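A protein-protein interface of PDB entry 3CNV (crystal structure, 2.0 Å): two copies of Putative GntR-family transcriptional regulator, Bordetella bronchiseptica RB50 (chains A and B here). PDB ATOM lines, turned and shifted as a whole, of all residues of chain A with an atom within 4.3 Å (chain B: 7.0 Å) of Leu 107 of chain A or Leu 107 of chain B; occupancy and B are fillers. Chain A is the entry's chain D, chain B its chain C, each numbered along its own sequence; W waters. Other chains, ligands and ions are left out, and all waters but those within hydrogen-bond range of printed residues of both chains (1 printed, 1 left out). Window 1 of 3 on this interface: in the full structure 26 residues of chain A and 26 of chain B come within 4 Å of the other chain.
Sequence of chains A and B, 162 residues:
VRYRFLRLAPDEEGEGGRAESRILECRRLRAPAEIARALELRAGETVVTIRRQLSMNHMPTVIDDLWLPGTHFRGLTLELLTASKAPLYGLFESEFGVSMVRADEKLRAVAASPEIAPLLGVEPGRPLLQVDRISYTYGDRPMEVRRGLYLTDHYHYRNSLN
Glu 105 of chain A touches Tyr 157 of chain B, and with the chains exchanged Tyr 157 of chain A touches Glu 105 of chain B.
Lys 106 of chain A touches Tyr 157 of chain B, and with the chains exchanged Tyr 157 of chain A touches Lys 106 of chain B.
Leu 107 of chain A touches His 156 of chain B, and with the chains exchanged His 156 of chain A touches Leu 107 of chain B.
Arg 108 of chain A touches His 156 of chain B, and with the chains exchanged His 156 of chain A touches Arg 108 of chain B.
Of the 21 pairs that touch across the chains among the printed residues, 14 have their exchanged pair printed and touching as well.
Of the 19 printed residues of chain B, 13 touch a printed residue of chain A.
N of Tyr 157 of chain A lies within hydrogen-bond range of O of Leu 107 of chain B, at 2.8 Å.
OD1 of Asp 11 of chain B is in salt-bridge range of NH2 of Arg 108 of chain A (3.4 Å).
The side-chain hydroxyl (OH) of Tyr 157 of chain A is in hydrogen-bond range of the side-chain amide nitrogen (ND2) of Asn 159 of chain B.
The backbone carbonyl oxygen of Asn 159 of chain B sits at hydrogen-bond distance from the backbone NH of Glu 105 of chain A.
The backbone NH (N) of Tyr 157 of chain B lies within hydrogen-bond range of the backbone carbonyl oxygen (O) of Leu 107 of chain A (2.8 Å).
Of chain B, only Leu 107 (3.6 Å), His 156 (3.4 Å) and Tyr 157 (2.8 Å) come within 4 Å of Leu 107 of chain A.
Printed residues of chain A within 4 Å of Leu 107 of chain B: Leu 107, His 156 and Tyr 157.
Printed residues of chain A within 4 Å of Arg 158 of chain B: Glu 105 (3.5 Å).
Of the printed residues of chain B, Glu 105 of chain A touches Tyr 157 (3.9 Å), Arg 158 (3.5 Å), Asn 159 (2.7 Å) and Leu 161 (3.4 Å).
Of the printed residues of chain A, Asn 159 of chain B touches Glu 105 (2.7 Å) and Tyr 157 (3.0 Å).
Of the printed residues of chain B, Tyr 157 of chain A touches Glu 105 (3.8 Å), Lys 106 (3.6 Å), Leu 107 (2.8 Å) and Asn 159 (3.0 Å).
Val 131 of chain B touches none of the printed residues of chain A.
The nearest printed residue of chain A that does not touch Leu 107 of chain B is Leu 129 of chain A (4.3 Å).
Tyr 157 of chain B touches Glu 105 of chain A (O to O, 3.9 Å).
His 156 of chain B touches Lys 106 of chain A (CD2 to CG, 3.5 Å).
CA of Lys 106 of chain A touches O of Tyr 157 of chain B, 3.5 Å away.
Leu 107 of chain B touches Leu 107 of chain A (CD2 to CD2, 3.6 Å).
Arg 108 of chain A touches His 156 of chain B.
Leu 129 of chain B touches Leu 129 of chain A.
Lys 106 of chain B touches His 156 of chain A.
NH2 of Arg 108 of chain B touches ND1 of His 156 of chain A (3.5 Å).
Glu 105 of chain B touches Tyr 157 of chain A (O to O, 3.8 Å).
Tyr 157 of chain A touches Lys 106 of chain B (O to CA, 3.6 Å).
The backbone NH (N) of Gln 130 of chain B sits at hydrogen-bond distance from the backbone carbonyl oxygen (O) of Arg 108 of chain B (2.7 Å).
OE1 of Glu 105 of chain B is in hydrogen-bond range of OH of Tyr 157 of chain B (2.4 Å).
O of Arg 108 of chain A lies within hydrogen-bond range of N of Gln 130 of chain A (2.8 Å).
The backbone NH of Asp 132 of chain B is in hydrogen-bond range of the backbone carbonyl oxygen of Lys 106 of chain B (2.8 Å).
The side-chain carboxylate of Asp 132 of chain B is in salt-bridge range of the guanidinium group of Arg 108 of chain B (2.8 Å).
OE1 of Glu 105 of chain A lies within hydrogen-bond range of OH of Tyr 157 of chain A.
Water W1 bridges the side-chain amino group (NZ) of Lys 106 of chain A (2.6 Å) and the backbone carbonyl oxygen (O) of Asp 11 of chain B (3.2 Å).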
ATOM      1  N   GLU A 105      20.491  -5.049   5.119  1.00  0.00           N
ATOM      2  CA  GLU A 105      21.780  -4.734   5.704  1.00  0.00           C
ATOM      3  C   GLU A 105      22.484  -3.649   4.965  1.00  0.00           C
ATOM      4  O   GLU A 105      22.279  -3.411   3.806  1.00  0.00           O
ATOM      5  CB  GLU A 105      22.721  -5.970   5.772  1.00  0.00           C
ATOM      6  CG  GLU A 105      22.206  -7.056   6.642  1.00  0.00           C
ATOM      7  CD  GLU A 105      23.092  -8.321   6.612  1.00  0.00           C
ATOM      8  OE1 GLU A 105      23.959  -8.504   5.714  1.00  0.00           O
ATOM      9  OE2 GLU A 105      22.898  -9.142   7.465  1.00  0.00           O
ATOM     10  N   LYS A 106      23.296  -2.949   5.725  1.00  0.00           N
ATOM     11  CA  LYS A 106      24.171  -1.916   5.188  1.00  0.00           C
ATOM     12  C   LYS A 106      25.534  -2.300   5.693  1.00  0.00           C
ATOM     13  O   LYS A 106      25.708  -2.401   6.886  1.00  0.00           O
ATOM     14  CB  LYS A 106      23.770  -0.533   5.710  1.00  0.00           C
ATOM     15  CG  LYS A 106      22.409  -0.049   5.253  1.00  0.00           C
ATOM     16  CD  LYS A 106      22.103   1.334   5.799  1.00  0.00           C
ATOM     17  CE  LYS A 106      20.744   1.751   5.317  1.00  0.00           C
ATOM     18  NZ  LYS A 106      20.404   3.160   5.640  1.00  0.00           N
ATOM     19  N   LEU A 107      26.457  -2.496   4.771  1.00  0.00           N
ATOM     20  CA  LEU A 107      27.837  -2.874   5.058  1.00  0.00           C
ATOM     21  C   LEU A 107      28.814  -1.743   4.739  1.00  0.00           C
ATOM     22  O   LEU A 107      28.699  -1.022   3.741  1.00  0.00           O
ATOM     23  CB  LEU A 107      28.249  -4.159   4.268  1.00  0.00           C
ATOM     24  CG  LEU A 107      27.587  -5.488   4.655  1.00  0.00           C
ATOM     25  CD1 LEU A 107      26.153  -5.629   4.260  1.00  0.00           C
ATOM     26  CD2 LEU A 107      28.413  -6.683   4.042  1.00  0.00           C
ATOM     27  N   ARG A 108      29.724  -1.591   5.681  1.00  0.00           N
ATOM     28  CA  ARG A 108      30.846  -0.627   5.599  1.00  0.00           C
ATOM     29  C   ARG A 108      32.101  -1.162   6.254  1.00  0.00           C
ATOM     30  O   ARG A 108      32.043  -1.970   7.150  1.00  0.00           O
ATOM     31  CB  ARG A 108      30.546   0.612   6.459  1.00  0.00           C
ATOM     32  CG  ARG A 108      29.371   1.372   6.043  1.00  0.00           C
ATOM     33  CD  ARG A 108      28.801   2.214   7.281  1.00  0.00           C
ATOM     34  NE  ARG A 108      27.572   2.926   6.877  1.00  0.00           N
ATOM     35  CZ  ARG A 108      26.343   2.555   7.194  1.00  0.00           C
ATOM     36  NH1 ARG A 108      26.099   1.504   7.965  1.00  0.00           N
ATOM     37  NH2 ARG A 108      25.341   3.266   6.751  1.00  0.00           N
ATOM     38  N   LEU A 129      34.660  -5.112   9.374  1.00  0.00           N
ATOM     39  CA  LEU A 129      33.438  -4.989   8.609  1.00  0.00           C
ATOM     40  C   LEU A 129      32.279  -4.745   9.549  1.00  0.00           C
ATOM     41  O   LEU A 129      31.967  -5.537  10.403  1.00  0.00           O
ATOM     42  CB  LEU A 129      33.235  -6.240   7.725  1.00  0.00           C
ATOM     43  CG  LEU A 129      31.993  -6.370   6.821  1.00  0.00           C
ATOM     44  CD1 LEU A 129      32.105  -5.323   5.705  1.00  0.00           C
ATOM     45  CD2 LEU A 129      31.878  -7.820   6.232  1.00  0.00           C
ATOM     46  N   GLN A 130      31.610  -3.636   9.338  1.00  0.00           N
ATOM     47  CA  GLN A 130      30.399  -3.304  10.072  1.00  0.00           C
ATOM     48  C   GLN A 130      29.153  -3.700   9.255  1.00  0.00           C
ATOM     49  O   GLN A 130      29.023  -3.296   8.123  1.00  0.00           O
ATOM     50  CB  GLN A 130      30.358  -1.838  10.366  1.00  0.00           C
ATOM     51  CG  GLN A 130      29.145  -1.467  11.182  1.00  0.00           C
ATOM     52  CD  GLN A 130      29.257  -0.006  11.680  1.00  0.00           C
ATOM     53  OE1 GLN A 130      29.952   0.236  12.615  1.00  0.00           O
ATOM     54  NE2 GLN A 130      28.652   0.930  10.987  1.00  0.00           N
ATOM     55  N   VAL A 131      28.293  -4.561   9.828  1.00  0.00           N
ATOM     56  CA  VAL A 131      27.042  -5.011   9.208  1.00  0.00           C
ATOM     57  C   VAL A 131      25.848  -4.488  10.054  1.00  0.00           C
ATOM     58  O   VAL A 131      25.617  -4.918  11.173  1.00  0.00           O
ATOM     59  CB  VAL A 131      27.026  -6.551   9.093  1.00  0.00           C
ATOM     60  CG1 VAL A 131      25.752  -7.044   8.462  1.00  0.00           C
ATOM     61  CG2 VAL A 131      28.269  -7.060   8.266  1.00  0.00           C
ATOM     62  N   HIS A 156      35.512 -14.319   5.635  1.00  0.00           N
ATOM     63  CA  HIS A 156      34.862 -13.267   4.845  1.00  0.00           C
ATOM     64  C   HIS A 156      33.346 -13.394   4.931  1.00  0.00           C
ATOM     65  O   HIS A 156      32.807 -14.407   5.378  1.00  0.00           O
ATOM     66  CB  HIS A 156      35.342 -13.341   3.382  1.00  0.00           C
ATOM     67  CG  HIS A 156      35.054 -14.647   2.709  1.00  0.00           C
ATOM     68  ND1 HIS A 156      35.925 -15.707   2.765  1.00  0.00           N
ATOM     69  CD2 HIS A 156      33.980 -15.070   2.010  1.00  0.00           C
ATOM     70  CE1 HIS A 156      35.394 -16.735   2.116  1.00  0.00           C
ATOM     71  NE2 HIS A 156      34.204 -16.376   1.665  1.00  0.00           N
ATOM     72  N   TYR A 157      32.689 -12.380   4.415  1.00  0.00           N
ATOM     73  CA  TYR A 157      31.237 -12.342   4.257  1.00  0.00           C
ATOM     74  C   TYR A 157      30.865 -12.757   2.837  1.00  0.00           C
ATOM     75  O   TYR A 157      31.244 -12.128   1.850  1.00  0.00           O
ATOM     76  CB  TYR A 157      30.751 -10.943   4.602  1.00  0.00           C
ATOM     77  CG  TYR A 157      29.298 -10.660   4.421  1.00  0.00           C
ATOM     78  CD1 TYR A 157      28.517 -10.293   5.504  1.00  0.00           C
ATOM     79  CD2 TYR A 157      28.702 -10.641   3.144  1.00  0.00           C
ATOM     80  CE1 TYR A 157      27.203  -9.967   5.354  1.00  0.00           C
ATOM     81  CE2 TYR A 157      27.356 -10.361   3.006  1.00  0.00           C
ATOM     82  CZ  TYR A 157      26.603 -10.029   4.143  1.00  0.00           C
ATOM     83  OH  TYR A 157      25.279  -9.632   4.009  1.00  0.00           O
ATOM     84  N   LEU B   8      26.632  -0.072  -4.024  1.00  0.00           N
ATOM     85  CA  LEU B   8      26.905   1.220  -3.383  1.00  0.00           C
ATOM     86  C   LEU B   8      25.657   2.103  -3.296  1.00  0.00           C
ATOM     87  O   LEU B   8      24.878   2.255  -4.241  1.00  0.00           O
ATOM     88  CB  LEU B   8      28.044   1.955  -4.066  1.00  0.00           C
ATOM     89  CG  LEU B   8      29.426   1.799  -3.416  1.00  0.00           C
ATOM     90  CD1 LEU B   8      30.177   3.018  -3.790  1.00  0.00           C
ATOM     91  CD2 LEU B   8      29.445   1.714  -1.878  1.00  0.00           C
ATOM     92  N   ASP B  11      24.841   7.258   2.103  1.00  0.00           N
ATOM     93  CA  ASP B  11      24.455   7.330   3.507  1.00  0.00           C
ATOM     94  C   ASP B  11      23.372   8.378   3.715  1.00  0.00           C
ATOM     95  O   ASP B  11      22.410   8.166   4.465  1.00  0.00           O
ATOM     96  CB  ASP B  11      25.662   7.636   4.412  1.00  0.00           C
ATOM     97  CG  ASP B  11      26.550   6.432   4.585  1.00  0.00           C
ATOM     98  OD1 ASP B  11      26.176   5.295   4.143  1.00  0.00           O
ATOM     99  OD2 ASP B  11      27.676   6.639   5.096  1.00  0.00           O
ATOM    100  N   ASP B 104      29.187 -14.200  -7.540  1.00  0.00           N
ATOM    101  CA  ASP B 104      29.475 -14.739  -6.207  1.00  0.00           C
ATOM    102  C   ASP B 104      30.566 -13.785  -5.653  1.00  0.00           C
ATOM    103  O   ASP B 104      31.543 -13.498  -6.327  1.00  0.00           O
ATOM    104  CB  ASP B 104      30.003 -16.146  -6.238  1.00  0.00           C
ATOM    105  CG  ASP B 104      28.966 -17.195  -6.686  1.00  0.00           C
ATOM    106  OD1 ASP B 104      27.707 -16.962  -6.551  1.00  0.00           O
ATOM    107  OD2 ASP B 104      29.438 -18.290  -7.156  1.00  0.00           O
ATOM    108  N   GLU B 105      30.324 -13.240  -4.474  1.00  0.00           N
ATOM    109  CA  GLU B 105      31.221 -12.276  -3.824  1.00  0.00           C
ATOM    110  C   GLU B 105      31.720 -12.723  -2.457  1.00  0.00           C
ATOM    111  O   GLU B 105      31.055 -13.430  -1.706  1.00  0.00           O
ATOM    112  CB  GLU B 105      30.563 -10.895  -3.726  1.00  0.00           C
ATOM    113  CG  GLU B 105      30.299 -10.223  -4.999  1.00  0.00           C
ATOM    114  CD  GLU B 105      29.581  -8.863  -4.865  1.00  0.00           C
ATOM    115  OE1 GLU B 105      29.067  -8.491  -3.779  1.00  0.00           O
ATOM    116  OE2 GLU B 105      29.486  -8.191  -5.897  1.00  0.00           O
ATOM    117  N   LYS B 106      32.923 -12.267  -2.145  1.00  0.00           N
ATOM    118  CA  LYS B 106      33.578 -12.413  -0.855  1.00  0.00           C
ATOM    119  C   LYS B 106      33.970 -10.992  -0.383  1.00  0.00           C
ATOM    120  O   LYS B 106      34.730 -10.270  -1.077  1.00  0.00           O
ATOM    121  CB  LYS B 106      34.825 -13.309  -0.974  1.00  0.00           C
ATOM    122  CG  LYS B 106      34.579 -14.701  -1.448  1.00  0.00           C
ATOM    123  CD  LYS B 106      35.857 -15.531  -1.477  1.00  0.00           C
ATOM    124  CE  LYS B 106      35.552 -17.002  -1.765  1.00  0.00           C
ATOM    125  NZ  LYS B 106      36.684 -17.911  -1.347  1.00  0.00           N
ATOM    126  N   LEU B 107      33.346 -10.563   0.718  1.00  0.00           N
ATOM    127  CA  LEU B 107      33.576  -9.227   1.320  1.00  0.00           C
ATOM    128  C   LEU B 107      34.369  -9.285   2.613  1.00  0.00           C
ATOM    129  O   LEU B 107      34.226 -10.180   3.477  1.00  0.00           O
ATOM    130  CB  LEU B 107      32.300  -8.465   1.547  1.00  0.00           C
ATOM    131  CG  LEU B 107      31.445  -7.935   0.391  1.00  0.00           C
ATOM    132  CD1 LEU B 107      30.876  -9.080  -0.511  1.00  0.00           C
ATOM    133  CD2 LEU B 107      30.363  -7.102   1.031  1.00  0.00           C
ATOM    134  N   ARG B 108      35.321  -8.373   2.646  1.00  0.00           N
ATOM    135  CA  ARG B 108      36.210  -8.189   3.809  1.00  0.00           C
ATOM    136  C   ARG B 108      36.578  -6.720   4.017  1.00  0.00           C
ATOM    137  O   ARG B 108      36.434  -5.895   3.126  1.00  0.00           O
ATOM    138  CB  ARG B 108      37.459  -9.105   3.729  1.00  0.00           C
ATOM    139  CG  ARG B 108      38.022  -9.481   2.330  1.00  0.00           C
ATOM    140  CD  ARG B 108      39.308 -10.431   2.285  1.00  0.00           C
ATOM    141  NE  ARG B 108      39.026 -11.878   2.232  1.00  0.00           N
ATOM    142  CZ  ARG B 108      38.667 -12.569   1.149  1.00  0.00           C
ATOM    143  NH1 ARG B 108      38.529 -11.997  -0.011  1.00  0.00           N
ATOM    144  NH2 ARG B 108      38.466 -13.851   1.231  1.00  0.00           N
ATOM    145  N   ALA B 109      37.023  -6.404   5.225  1.00  0.00           N
ATOM    146  CA  ALA B 109      37.590  -5.076   5.492  1.00  0.00           C
ATOM    147  C   ALA B 109      39.079  -5.202   5.532  1.00  0.00           C
ATOM    148  O   ALA B 109      39.632  -6.112   6.174  1.00  0.00           O
ATOM    149  CB  ALA B 109      37.067  -4.423   6.811  1.00  0.00           C
ATOM    150  N   LEU B 129      36.426  -1.379   2.201  1.00  0.00           N
ATOM    151  CA  LEU B 129      35.589  -2.580   1.953  1.00  0.00           C
ATOM    152  C   LEU B 129      36.104  -3.234   0.666  1.00  0.00           C
ATOM    153  O   LEU B 129      36.165  -2.621  -0.395  1.00  0.00           O
ATOM    154  CB  LEU B 129      34.134  -2.263   1.832  1.00  0.00           C
ATOM    155  CG  LEU B 129      33.179  -3.432   1.521  1.00  0.00           C
ATOM    156  CD1 LEU B 129      33.136  -4.446   2.674  1.00  0.00           C
ATOM    157  CD2 LEU B 129      31.813  -2.979   1.134  1.00  0.00           C
ATOM    158  N   GLN B 130      36.605  -4.448   0.819  1.00  0.00           N
ATOM    159  CA  GLN B 130      37.061  -5.217  -0.339  1.00  0.00           C
ATOM    160  C   GLN B 130      35.956  -6.190  -0.740  1.00  0.00           C
ATOM    161  O   GLN B 130      35.428  -6.964   0.066  1.00  0.00           O
ATOM    162  CB  GLN B 130      38.398  -5.905  -0.084  1.00  0.00           C
ATOM    163  CG  GLN B 130      38.867  -6.852  -1.203  1.00  0.00           C
ATOM    164  CD  GLN B 130      40.293  -7.383  -0.969  1.00  0.00           C
ATOM    165  OE1 GLN B 130      41.243  -6.622  -0.909  1.00  0.00           O
ATOM    166  NE2 GLN B 130      40.414  -8.663  -0.759  1.00  0.00           N
ATOM    167  N   VAL B 131      35.571  -6.081  -1.997  1.00  0.00           N
ATOM    168  CA  VAL B 131      34.544  -6.924  -2.626  1.00  0.00           C
ATOM    169  C   VAL B 131      35.245  -7.731  -3.746  1.00  0.00           C
ATOM    170  O   VAL B 131      35.594  -7.222  -4.810  1.00  0.00           O
ATOM    171  CB  VAL B 131      33.344  -6.115  -3.208  1.00  0.00           C
ATOM    172  CG1 VAL B 131      32.259  -7.086  -3.798  1.00  0.00           C
ATOM    173  CG2 VAL B 131      32.686  -5.134  -2.119  1.00  0.00           C
ATOM    174  N   ASP B 132      35.471  -9.009  -3.489  1.00  0.00           N
ATOM    175  CA  ASP B 132      36.009  -9.899  -4.511  1.00  0.00           C
ATOM    176  C   ASP B 132      34.875 -10.671  -5.215  1.00  0.00           C
ATOM    177  O   ASP B 132      34.183 -11.460  -4.590  1.00  0.00           O
ATOM    178  CB  ASP B 132      37.006 -10.899  -3.864  1.00  0.00           C
ATOM    179  CG  ASP B 132      38.335 -10.239  -3.470  1.00  0.00           C
ATOM    180  OD1 ASP B 132      38.867  -9.431  -4.266  1.00  0.00           O
ATOM    181  OD2 ASP B 132      38.829 -10.480  -2.339  1.00  0.00           O
ATOM    182  N   THR B 152      34.042   3.595   2.083  1.00  0.00           N
ATOM    183  CA  THR B 152      32.666   3.586   2.572  1.00  0.00           C
ATOM    184  C   THR B 152      32.400   4.678   3.589  1.00  0.00           C
ATOM    185  O   THR B 152      31.673   4.480   4.544  1.00  0.00           O
ATOM    186  CB  THR B 152      32.280   2.189   3.142  1.00  0.00           C
ATOM    187  OG1 THR B 152      33.171   1.831   4.188  1.00  0.00           O
ATOM    188  CG2 THR B 152      32.376   1.183   2.118  1.00  0.00           C
ATOM    189  N   TYR B 155      29.136   6.301   1.653  1.00  0.00           N
ATOM    190  CA  TYR B 155      28.405   5.291   0.929  1.00  0.00           C
ATOM    191  C   TYR B 155      28.575   3.942   1.696  1.00  0.00           C
ATOM    192  O   TYR B 155      29.494   3.739   2.514  1.00  0.00           O
ATOM    193  CB  TYR B 155      28.901   5.176  -0.508  1.00  0.00           C
ATOM    194  CG  TYR B 155      28.461   6.287  -1.470  1.00  0.00           C
ATOM    195  CD1 TYR B 155      27.411   6.106  -2.285  1.00  0.00           C
ATOM    196  CD2 TYR B 155      29.118   7.526  -1.501  1.00  0.00           C
ATOM    197  CE1 TYR B 155      26.980   7.122  -3.133  1.00  0.00           C
ATOM    198  CE2 TYR B 155      28.681   8.562  -2.327  1.00  0.00           C
ATOM    199  CZ  TYR B 155      27.620   8.320  -3.162  1.00  0.00           C
ATOM    200  OH  TYR B 155      27.138   9.277  -4.019  1.00  0.00           O
ATOM    201  N   HIS B 156      27.582   3.095   1.541  1.00  0.00           N
ATOM    202  CA  HIS B 156      27.574   1.750   2.118  1.00  0.00           C
ATOM    203  C   HIS B 156      27.243   0.772   0.998  1.00  0.00           C
ATOM    204  O   HIS B 156      26.753   1.170  -0.059  1.00  0.00           O
ATOM    205  CB  HIS B 156      26.571   1.639   3.324  1.00  0.00           C
ATOM    206  CG  HIS B 156      25.149   1.993   2.996  1.00  0.00           C
ATOM    207  ND1 HIS B 156      24.684   3.282   3.102  1.00  0.00           N
ATOM    208  CD2 HIS B 156      24.107   1.254   2.520  1.00  0.00           C
ATOM    209  CE1 HIS B 156      23.421   3.330   2.708  1.00  0.00           C
ATOM    210  NE2 HIS B 156      23.048   2.125   2.330  1.00  0.00           N
ATOM    211  N   TYR B 157      27.475  -0.502   1.280  1.00  0.00           N
ATOM    212  CA  TYR B 157      27.026  -1.609   0.428  1.00  0.00           C
ATOM    213  C   TYR B 157      25.699  -2.139   1.005  1.00  0.00           C
ATOM    214  O   TYR B 157      25.637  -2.610   2.086  1.00  0.00           O
ATOM    215  CB  TYR B 157      28.140  -2.689   0.417  1.00  0.00           C
ATOM    216  CG  TYR B 157      27.877  -3.973  -0.282  1.00  0.00           C
ATOM    217  CD1 TYR B 157      28.643  -4.322  -1.365  1.00  0.00           C
ATOM    218  CD2 TYR B 157      26.936  -4.854   0.158  1.00  0.00           C
ATOM    219  CE1 TYR B 157      28.471  -5.470  -2.041  1.00  0.00           C
ATOM    220  CE2 TYR B 157      26.704  -6.098  -0.562  1.00  0.00           C
ATOM    221  CZ  TYR B 157      27.517  -6.387  -1.645  1.00  0.00           C
ATOM    222  OH  TYR B 157      27.362  -7.596  -2.335  1.00  0.00           O
ATOM    223  N   ARG B 158      24.661  -2.034   0.211  1.00  0.00           N
ATOM    224  CA  ARG B 158      23.286  -2.420   0.553  1.00  0.00           C
ATOM    225  C   ARG B 158      23.050  -3.841   0.166  1.00  0.00           C
ATOM    226  O   ARG B 158      23.403  -4.240  -0.930  1.00  0.00           O
ATOM    227  CB  ARG B 158      22.252  -1.507  -0.142  1.00  0.00           C
ATOM    228  CG  ARG B 158      22.205  -1.682  -1.674  1.00  0.00           C
ATOM    229  CD  ARG B 158      21.189  -0.723  -2.348  1.00  0.00           C
ATOM    230  NE  ARG B 158      21.154  -0.844  -3.800  1.00  0.00           N
ATOM    231  CZ  ARG B 158      20.994  -1.984  -4.502  1.00  0.00           C
ATOM    232  NH1 ARG B 158      20.912  -3.199  -3.920  1.00  0.00           N
ATOM    233  NH2 ARG B 158      20.961  -1.888  -5.824  1.00  0.00           N
ATOM    234  N   ASN B 159      22.497  -4.623   1.082  1.00  0.00           N
ATOM    235  CA  ASN B 159      22.225  -6.026   0.817  1.00  0.00           C
ATOM    236  C   ASN B 159      20.899  -6.435   1.465  1.00  0.00           C
ATOM    237  O   ASN B 159      20.746  -6.290   2.681  1.00  0.00           O
ATOM    238  CB  ASN B 159      23.329  -6.973   1.358  1.00  0.00           C
ATOM    239  CG  ASN B 159      23.287  -8.378   0.712  1.00  0.00           C
ATOM    240  OD1 ASN B 159      22.837  -8.562  -0.439  1.00  0.00           O
ATOM    241  ND2 ASN B 159      23.854  -9.344   1.420  1.00  0.00           N
ATOM    242  N   LEU B 161      18.541  -9.742   2.283  1.00  0.00           N
ATOM    243  CA  LEU B 161      18.704 -11.178   2.472  1.00  0.00           C
ATOM    244  C   LEU B 161      17.356 -11.836   2.727  1.00  0.00           C
ATOM    245  O   LEU B 161      16.566 -11.347   3.504  1.00  0.00           O
ATOM    246  CB  LEU B 161      19.562 -11.454   3.704  1.00  0.00           C
ATOM    247  CG  LEU B 161      21.001 -10.945   3.785  1.00  0.00           C
ATOM    248  CD1 LEU B 161      21.028  -9.414   4.171  1.00  0.00           C
ATOM    249  CD2 LEU B 161      21.654 -11.748   4.897  1.00  0.00           C
HETATM  250  O   HOH W   1      22.093   5.077   5.309  1.00  0.00           O
